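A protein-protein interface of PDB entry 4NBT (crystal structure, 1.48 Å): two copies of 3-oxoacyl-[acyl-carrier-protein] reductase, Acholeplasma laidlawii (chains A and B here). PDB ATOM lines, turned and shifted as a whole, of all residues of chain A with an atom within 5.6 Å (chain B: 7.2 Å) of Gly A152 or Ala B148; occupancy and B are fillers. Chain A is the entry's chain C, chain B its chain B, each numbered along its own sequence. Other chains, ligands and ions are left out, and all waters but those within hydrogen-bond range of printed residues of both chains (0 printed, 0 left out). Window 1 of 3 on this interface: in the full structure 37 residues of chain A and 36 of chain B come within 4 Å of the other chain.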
ATOM      1  N   LEU A 106      -2.216   2.681 -14.224  1.00  0.00           N
ATOM      2  CA  LEU A 106      -0.838   2.519 -13.788  1.00  0.00           C
ATOM      3  C   LEU A 106      -0.809   1.540 -12.631  1.00  0.00           C
ATOM      4  O   LEU A 106      -0.236   0.460 -12.744  1.00  0.00           O
ATOM      5  CB  LEU A 106      -0.205   3.877 -13.464  1.00  0.00           C
ATOM      6  CG  LEU A 106       1.310   3.922 -13.430  1.00  0.00           C
ATOM      7  CD1 LEU A 106       1.899   3.629 -14.792  1.00  0.00           C
ATOM      8  CD2 LEU A 106       1.788   5.292 -12.944  1.00  0.00           C
ATOM      9  N   ALA A 147      -1.910  10.719 -20.061  1.00  0.00           N
ATOM     10  CA  ALA A 147      -0.569  10.721 -20.634  1.00  0.00           C
ATOM     11  C   ALA A 147       0.478  10.250 -19.621  1.00  0.00           C
ATOM     12  O   ALA A 147       1.386   9.506 -19.965  1.00  0.00           O
ATOM     13  CB  ALA A 147      -0.230  12.090 -21.147  1.00  0.00           C
ATOM     14  N   ALA A 148       0.365  10.693 -18.370  1.00  0.00           N
ATOM     15  CA  ALA A 148       1.276  10.229 -17.318  1.00  0.00           C
ATOM     16  C   ALA A 148       1.220   8.725 -17.189  1.00  0.00           C
ATOM     17  O   ALA A 148       2.245   8.064 -17.076  1.00  0.00           O
ATOM     18  CB  ALA A 148       0.944  10.887 -15.984  1.00  0.00           C
ATOM     19  N   THR A 149       0.018   8.170 -17.244  1.00  0.00           N
ATOM     20  CA  THR A 149      -0.108   6.718 -17.095  1.00  0.00           C
ATOM     21  C   THR A 149       0.424   5.972 -18.312  1.00  0.00           C
ATOM     22  O   THR A 149       1.081   4.947 -18.156  1.00  0.00           O
ATOM     23  CB  THR A 149      -1.554   6.252 -16.786  1.00  0.00           C
ATOM     24  OG1 THR A 149      -2.420   6.400 -17.928  1.00  0.00           O
ATOM     25  CG2 THR A 149      -2.094   6.968 -15.539  1.00  0.00           C
ATOM     26  N   LYS A 150       0.166   6.488 -19.505  1.00  0.00           N
ATOM     27  CA  LYS A 150       0.523   5.743 -20.696  1.00  0.00           C
ATOM     28  C   LYS A 150       2.027   5.851 -20.996  1.00  0.00           C
ATOM     29  O   LYS A 150       2.624   4.927 -21.539  1.00  0.00           O
ATOM     30  CB  LYS A 150      -0.372   6.160 -21.864  1.00  0.00           C
ATOM     31  CG  LYS A 150      -1.850   5.831 -21.632  1.00  0.00           C
ATOM     32  CD  LYS A 150      -2.045   4.343 -21.349  1.00  0.00           C
ATOM     33  CE  LYS A 150      -3.484   3.872 -21.548  1.00  0.00           C
ATOM     34  NZ  LYS A 150      -3.586   2.422 -21.289  1.00  0.00           N
ATOM     35  N   ALA A 151       2.643   6.967 -20.625  1.00  0.00           N
ATOM     36  CA  ALA A 151       4.094   7.053 -20.641  1.00  0.00           C
ATOM     37  C   ALA A 151       4.664   6.206 -19.513  1.00  0.00           C
ATOM     38  O   ALA A 151       5.674   5.526 -19.673  1.00  0.00           O
ATOM     39  CB  ALA A 151       4.534   8.482 -20.529  1.00  0.00           C
ATOM     40  N   GLY A 152       4.012   6.228 -18.351  1.00  0.00           N
ATOM     41  CA  GLY A 152       4.472   5.426 -17.235  1.00  0.00           C
ATOM     42  C   GLY A 152       4.538   3.935 -17.518  1.00  0.00           C
ATOM     43  O   GLY A 152       5.445   3.239 -17.068  1.00  0.00           O
ATOM     44  N   VAL A 153       3.561   3.454 -18.275  1.00  0.00           N
ATOM     45  CA  VAL A 153       3.515   2.061 -18.691  1.00  0.00           C
ATOM     46  C   VAL A 153       4.752   1.662 -19.481  1.00  0.00           C
ATOM     47  O   VAL A 153       5.178   0.506 -19.440  1.00  0.00           O
ATOM     48  CB  VAL A 153       2.203   1.816 -19.509  1.00  0.00           C
ATOM     49  CG1 VAL A 153       2.337   0.656 -20.488  1.00  0.00           C
ATOM     50  CG2 VAL A 153       1.036   1.679 -18.543  1.00  0.00           C
ATOM     51  N   ILE A 154       5.321   2.597 -20.221  1.00  0.00           N
ATOM     52  CA  ILE A 154       6.548   2.321 -20.961  1.00  0.00           C
ATOM     53  C   ILE A 154       7.707   2.099 -19.976  1.00  0.00           C
ATOM     54  O   ILE A 154       8.543   1.190 -20.169  1.00  0.00           O
ATOM     55  CB  ILE A 154       6.830   3.441 -21.976  1.00  0.00           C
ATOM     56  CG1 ILE A 154       5.662   3.522 -22.973  1.00  0.00           C
ATOM     57  CG2 ILE A 154       8.170   3.199 -22.656  1.00  0.00           C
ATOM     58  CD1 ILE A 154       5.702   4.722 -23.917  1.00  0.00           C
ATOM     59  N   GLY A 155       7.758   2.891 -18.891  1.00  0.00           N
ATOM     60  CA  GLY A 155       8.746   2.665 -17.848  1.00  0.00           C
ATOM     61  C   GLY A 155       8.617   1.306 -17.188  1.00  0.00           C
ATOM     62  O   GLY A 155       9.614   0.640 -16.932  1.00  0.00           O
ATOM     63  N   LEU A 156       7.381   0.891 -16.928  1.00  0.00           N
ATOM     64  CA  LEU A 156       7.122  -0.437 -16.380  1.00  0.00           C
ATOM     65  C   LEU A 156       7.586  -1.498 -17.356  1.00  0.00           C
ATOM     66  O   LEU A 156       8.190  -2.510 -16.988  1.00  0.00           O
ATOM     67  CB  LEU A 156       5.626  -0.626 -16.115  1.00  0.00           C
ATOM     68  CG  LEU A 156       5.035   0.213 -14.984  1.00  0.00           C
ATOM     69  CD1 LEU A 156       3.535  -0.041 -14.911  1.00  0.00           C
ATOM     70  CD2 LEU A 156       5.699  -0.113 -13.637  1.00  0.00           C
ATOM     71  N   THR A 157       7.261  -1.293 -18.622  1.00  0.00           N
ATOM     72  CA  THR A 157       7.564  -2.268 -19.666  1.00  0.00           C
ATOM     73  C   THR A 157       9.064  -2.571 -19.729  1.00  0.00           C
ATOM     74  O   THR A 157       9.502  -3.722 -19.734  1.00  0.00           O
ATOM     75  CB  THR A 157       7.046  -1.754 -21.044  1.00  0.00           C
ATOM     76  OG1 THR A 157       5.613  -1.682 -21.019  1.00  0.00           O
ATOM     77  CG2 THR A 157       7.469  -2.678 -22.170  1.00  0.00           C
ATOM     78  N   TRP B  98       5.085   1.162  -3.624  1.00  0.00           N
ATOM     79  CA  TRP B  98       4.490   1.657  -4.841  1.00  0.00           C
ATOM     80  C   TRP B  98       3.843   3.007  -4.609  1.00  0.00           C
ATOM     81  O   TRP B  98       4.164   4.001  -5.290  1.00  0.00           O
ATOM     82  CB  TRP B  98       3.442   0.656  -5.383  1.00  0.00           C
ATOM     83  CG  TRP B  98       2.696   1.247  -6.556  1.00  0.00           C
ATOM     84  CD1 TRP B  98       1.562   1.991  -6.514  1.00  0.00           C
ATOM     85  CD2 TRP B  98       3.094   1.207  -7.934  1.00  0.00           C
ATOM     86  NE1 TRP B  98       1.242   2.446  -7.767  1.00  0.00           N
ATOM     87  CE2 TRP B  98       2.149   1.946  -8.660  1.00  0.00           C
ATOM     88  CE3 TRP B  98       4.161   0.619  -8.620  1.00  0.00           C
ATOM     89  CZ2 TRP B  98       2.232   2.102 -10.046  1.00  0.00           C
ATOM     90  CZ3 TRP B  98       4.232   0.768  -9.984  1.00  0.00           C
ATOM     91  CH2 TRP B  98       3.288   1.510 -10.676  1.00  0.00           C
ATOM     92  N   VAL B 101       5.939   6.356  -3.882  1.00  0.00           N
ATOM     93  CA  VAL B 101       6.754   6.846  -4.988  1.00  0.00           C
ATOM     94  C   VAL B 101       5.858   7.507  -6.049  1.00  0.00           C
ATOM     95  O   VAL B 101       6.192   8.556  -6.569  1.00  0.00           O
ATOM     96  CB  VAL B 101       7.623   5.715  -5.573  1.00  0.00           C
ATOM     97  CG1 VAL B 101       8.265   6.115  -6.900  1.00  0.00           C
ATOM     98  CG2 VAL B 101       8.667   5.279  -4.570  1.00  0.00           C
ATOM     99  N   ILE B 102       4.718   6.908  -6.372  1.00  0.00           N
ATOM    100  CA  ILE B 102       3.814   7.523  -7.324  1.00  0.00           C
ATOM    101  C   ILE B 102       3.268   8.852  -6.778  1.00  0.00           C
ATOM    102  O   ILE B 102       3.132   9.831  -7.510  1.00  0.00           O
ATOM    103  CB  ILE B 102       2.661   6.558  -7.721  1.00  0.00           C
ATOM    104  CG1 ILE B 102       3.092   5.618  -8.851  1.00  0.00           C
ATOM    105  CG2 ILE B 102       1.432   7.340  -8.194  1.00  0.00           C
ATOM    106  CD1 ILE B 102       4.261   4.726  -8.561  1.00  0.00           C
ATOM    107  N   ASN B 105       6.359  11.451  -6.821  1.00  0.00           N
ATOM    108  CA  ASN B 105       7.061  11.669  -8.082  1.00  0.00           C
ATOM    109  C   ASN B 105       6.151  11.961  -9.253  1.00  0.00           C
ATOM    110  O   ASN B 105       6.616  12.448 -10.280  1.00  0.00           O
ATOM    111  CB  ASN B 105       7.909  10.464  -8.439  1.00  0.00           C
ATOM    112  CG  ASN B 105       9.057  10.211  -7.484  1.00  0.00           C
ATOM    113  OD1 ASN B 105       9.166  10.795  -6.393  1.00  0.00           O
ATOM    114  ND2 ASN B 105       9.918   9.272  -7.879  1.00  0.00           N
ATOM    115  N   LEU B 106       4.875  11.615  -9.146  1.00  0.00           N
ATOM    116  CA  LEU B 106       3.921  11.862 -10.209  1.00  0.00           C
ATOM    117  C   LEU B 106       2.814  12.764  -9.709  1.00  0.00           C
ATOM    118  O   LEU B 106       2.645  13.869 -10.218  1.00  0.00           O
ATOM    119  CB  LEU B 106       3.355  10.542 -10.738  1.00  0.00           C
ATOM    120  CG  LEU B 106       2.960  10.434 -12.193  1.00  0.00           C
ATOM    121  CD1 LEU B 106       4.042  10.913 -13.183  1.00  0.00           C
ATOM    122  CD2 LEU B 106       2.608   8.966 -12.445  1.00  0.00           C
ATOM    123  N   VAL B 135      16.460   6.288 -15.590  1.00  0.00           N
ATOM    124  CA  VAL B 135      15.622   5.137 -15.257  1.00  0.00           C
ATOM    125  C   VAL B 135      14.263   5.228 -15.933  1.00  0.00           C
ATOM    126  O   VAL B 135      13.683   4.200 -16.291  1.00  0.00           O
ATOM    127  CB  VAL B 135      15.504   5.005 -13.740  1.00  0.00           C
ATOM    128  CG1 VAL B 135      14.566   3.841 -13.355  1.00  0.00           C
ATOM    129  CG2 VAL B 135      16.914   4.787 -13.160  1.00  0.00           C
ATOM    130  N   GLY B 136      13.755   6.443 -16.132  1.00  0.00           N
ATOM    131  CA  GLY B 136      12.520   6.616 -16.876  1.00  0.00           C
ATOM    132  C   GLY B 136      12.689   6.366 -18.372  1.00  0.00           C
ATOM    133  O   GLY B 136      11.725   6.047 -19.051  1.00  0.00           O
ATOM    134  N   GLN B 143      13.283  -1.117  -9.686  1.00  0.00           N
ATOM    135  CA  GLN B 143      12.743   0.236  -9.652  1.00  0.00           C
ATOM    136  C   GLN B 143      11.515   0.440 -10.510  1.00  0.00           C
ATOM    137  O   GLN B 143      11.331   1.510 -11.085  1.00  0.00           O
ATOM    138  CB  GLN B 143      13.819   1.235 -10.070  1.00  0.00           C
ATOM    139  CG  GLN B 143      15.026   1.244  -9.156  1.00  0.00           C
ATOM    140  CD  GLN B 143      15.866   2.485  -9.345  1.00  0.00           C
ATOM    141  OE1 GLN B 143      16.500   2.662 -10.394  1.00  0.00           O
ATOM    142  NE2 GLN B 143      15.851   3.374  -8.355  1.00  0.00           N
ATOM    143  N   ALA B 144      10.634  -0.555 -10.553  1.00  0.00           N
ATOM    144  CA  ALA B 144       9.437  -0.419 -11.367  1.00  0.00           C
ATOM    145  C   ALA B 144       8.608   0.819 -10.991  1.00  0.00           C
ATOM    146  O   ALA B 144       8.100   1.530 -11.877  1.00  0.00           O
ATOM    147  CB  ALA B 144       8.582  -1.667 -11.295  1.00  0.00           C
ATOM    148  N   ASN B 145       8.437   1.059  -9.682  1.00  0.00           N
ATOM    149  CA  ASN B 145       7.700   2.235  -9.242  1.00  0.00           C
ATOM    150  C   ASN B 145       8.370   3.543  -9.695  1.00  0.00           C
ATOM    151  O   ASN B 145       7.722   4.426 -10.292  1.00  0.00           O
ATOM    152  CB  ASN B 145       7.466   2.200  -7.717  1.00  0.00           C
ATOM    153  CG  ASN B 145       8.733   1.946  -6.905  1.00  0.00           C
ATOM    154  OD1 ASN B 145       9.810   1.699  -7.439  1.00  0.00           O
ATOM    155  ND2 ASN B 145       8.589   1.994  -5.568  1.00  0.00           N
ATOM    156  N   TYR B 146       9.670   3.661  -9.438  1.00  0.00           N
ATOM    157  CA  TYR B 146      10.421   4.852  -9.831  1.00  0.00           C
ATOM    158  C   TYR B 146      10.399   5.040 -11.350  1.00  0.00           C
ATOM    159  O   TYR B 146      10.141   6.156 -11.833  1.00  0.00           O
ATOM    160  CB  TYR B 146      11.852   4.748  -9.313  1.00  0.00           C
ATOM    161  CG  TYR B 146      12.691   5.979  -9.483  1.00  0.00           C
ATOM    162  CD1 TYR B 146      12.514   7.088  -8.676  1.00  0.00           C
ATOM    163  CD2 TYR B 146      13.677   6.026 -10.443  1.00  0.00           C
ATOM    164  CE1 TYR B 146      13.291   8.196  -8.816  1.00  0.00           C
ATOM    165  CE2 TYR B 146      14.461   7.128 -10.588  1.00  0.00           C
ATOM    166  CZ  TYR B 146      14.264   8.209  -9.768  1.00  0.00           C
ATOM    167  OH  TYR B 146      15.068   9.315  -9.935  1.00  0.00           O
ATOM    168  N   ALA B 147      10.658   3.969 -12.091  1.00  0.00           N
ATOM    169  CA  ALA B 147      10.650   4.052 -13.545  1.00  0.00           C
ATOM    170  C   ALA B 147       9.295   4.501 -14.081  1.00  0.00           C
ATOM    171  O   ALA B 147       9.215   5.305 -15.010  1.00  0.00           O
ATOM    172  CB  ALA B 147      11.034   2.726 -14.155  1.00  0.00           C
ATOM    173  N   ALA B 148       8.222   3.949 -13.537  1.00  0.00           N
ATOM    174  CA  ALA B 148       6.890   4.377 -13.933  1.00  0.00           C
ATOM    175  C   ALA B 148       6.724   5.873 -13.750  1.00  0.00           C
ATOM    176  O   ALA B 148       6.181   6.554 -14.613  1.00  0.00           O
ATOM    177  CB  ALA B 148       5.826   3.602 -13.150  1.00  0.00           C
ATOM    178  N   THR B 149       7.192   6.403 -12.621  1.00  0.00           N
ATOM    179  CA  THR B 149       7.016   7.832 -12.384  1.00  0.00           C
ATOM    180  C   THR B 149       7.886   8.692 -13.292  1.00  0.00           C
ATOM    181  O   THR B 149       7.445   9.732 -13.754  1.00  0.00           O
ATOM    182  CB  THR B 149       7.226   8.253 -10.902  1.00  0.00           C
ATOM    183  OG1 THR B 149       8.608   8.143 -10.512  1.00  0.00           O
ATOM    184  CG2 THR B 149       6.307   7.443  -9.986  1.00  0.00           C
ATOM    185  N   LYS B 150       9.118   8.264 -13.556  1.00  0.00           N
ATOM    186  CA  LYS B 150      10.039   9.127 -14.283  1.00  0.00           C
ATOM    187  C   LYS B 150       9.758   9.058 -15.791  1.00  0.00           C
ATOM    188  O   LYS B 150       9.948  10.037 -16.524  1.00  0.00           O
ATOM    189  CB  LYS B 150      11.485   8.808 -13.920  1.00  0.00           C
ATOM    190  CG  LYS B 150      11.848   9.134 -12.450  1.00  0.00           C
ATOM    191  CD  LYS B 150      11.481  10.554 -12.082  1.00  0.00           C
ATOM    192  CE  LYS B 150      12.110  11.014 -10.781  1.00  0.00           C
ATOM    193  NZ  LYS B 150      11.862  12.456 -10.557  1.00  0.00           N
ATOM    194  N   ALA B 151       9.212   7.939 -16.247  1.00  0.00           N
ATOM    195  CA  ALA B 151       8.660   7.877 -17.604  1.00  0.00           C
ATOM    196  C   ALA B 151       7.361   8.685 -17.666  1.00  0.00           C
ATOM    197  O   ALA B 151       7.114   9.423 -18.633  1.00  0.00           O
ATOM    198  CB  ALA B 151       8.398   6.420 -18.020  1.00  0.00           C
ATOM    199  N   GLY B 152       6.525   8.570 -16.631  1.00  0.00           N
ATOM    200  CA  GLY B 152       5.278   9.321 -16.589  1.00  0.00           C
ATOM    201  C   GLY B 152       5.466  10.823 -16.667  1.00  0.00           C
ATOM    202  O   GLY B 152       4.680  11.541 -17.271  1.00  0.00           O
ATOM    203  N   VAL B 153       6.537  11.298 -16.059  1.00  0.00           N
ATOM    204  CA  VAL B 153       6.869  12.715 -16.067  1.00  0.00           C
ATOM    205  C   VAL B 153       7.120  13.213 -17.484  1.00  0.00           C
ATOM    206  O   VAL B 153       6.867  14.383 -17.797  1.00  0.00           O
ATOM    207  CB  VAL B 153       8.128  12.970 -15.177  1.00  0.00           C
ATOM    208  CG1 VAL B 153       8.884  14.240 -15.576  1.00  0.00           C
ATOM    209  CG2 VAL B 153       7.713  12.960 -13.713  1.00  0.00           C
ATOM    210  N   ILE B 154       7.630  12.346 -18.342  1.00  0.00           N
ATOM    211  CA  ILE B 154       7.812  12.703 -19.748  1.00  0.00           C
ATOM    212  C   ILE B 154       6.441  12.909 -20.411  1.00  0.00           C
ATOM    213  O   ILE B 154       6.233  13.867 -21.166  1.00  0.00           O
ATOM    214  CB  ILE B 154       8.672  11.678 -20.482  1.00  0.00           C
ATOM    215  CG1 ILE B 154      10.061  11.620 -19.825  1.00  0.00           C
ATOM    216  CG2 ILE B 154       8.767  12.031 -21.948  1.00  0.00           C
ATOM    217  CD1 ILE B 154      10.985  10.504 -20.319  1.00  0.00           C
ATOM    218  N   GLY B 155       5.476  12.043 -20.112  1.00  0.00           N
ATOM    219  CA  GLY B 155       4.106  12.224 -20.585  1.00  0.00           C
ATOM    220  C   GLY B 155       3.507  13.545 -20.133  1.00  0.00           C
ATOM    221  O   GLY B 155       2.844  14.251 -20.899  1.00  0.00           O
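Trp B98 touches Leu A106 (CZ2 to CG, 3.95 Å).
Leu B106 touches Leu A106 (CD2 to CD2, 3.8 Å).
O of Gly B155 touches CB of Ala A147 (3.8 Å).
Ala A151 touches Ala B151.
Ala A151 touches Gly B155 (CB to N, 3.7 Å).
Ala B148 touches Gly A152.
Gly B152 touches Gly A152.
Ala B147 touches Gly A155.
Gly A155 touches Ala B151.
O of Ala B144 touches CD2 of Leu A156 (3.4 Å).
Printed residues of chain B within 4 Å of Ala A148: Gly B152.
Of chain B, only Ala B148 and Gly B152 come within 4 Å of Gly A152.
Of the printed residues of chain B, Gly A155 touches Ala B147 and Ala B151.
Gln B143 touches none of the printed residues of chain A.
Asn B145 touches none of the printed residues of chain A.
Ala B148 touches two residues of chain A.
Of the printed residues of chain A, Gly B152 touches Ala A148 and Gly A152.
Of the printed residues of chain A, Gly B155 touches Ala A147 (3.8 Å) and Ala A151 (3.7 Å).
The nearest residue of chain B that does not touch Gly A152 is Ala B151 (4.1 Å).
The nearest residue of chain A that does not touch Ala B148 is Leu A106 (4.3 Å).
The nearest printed residue of chain A that does not touch Trp B98 is Leu A156 (4.03 Å).
Of the 20 printed residues of chain B, 8 touch a printed residue of chain A.
Hydrophobic or aromatic side chains of chain A that line the printed part of chain B: Leu A106, Ala A147, Ala A151 and Leu A156.
Among the printed residues, 12 pairs touch across the chains.
Among the printed residues, no Asp or Glu carboxylate lies within 4 Å of a Lys or Arg side-chain nitrogen of the other chain.
Ala A147 touches Gly B155, and with the chains exchanged Gly A155 touches Ala B147.
Ala A148 touches Gly B152, and with the chains exchanged Gly A152 touches Ala B148.
Ala A151 touches Gly B155, and with the chains exchanged Gly A155 touches Ala B151.
Gly B152 touches its own counterpart, Gly A152.
Positions printed for both chains: 106, 147, 148, 149, 150, 151, 152, 153, 154 and 155.
Of the 12 pairs that touch across the chains among the printed residues, 9 have their exchanged pair printed and touching as well.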
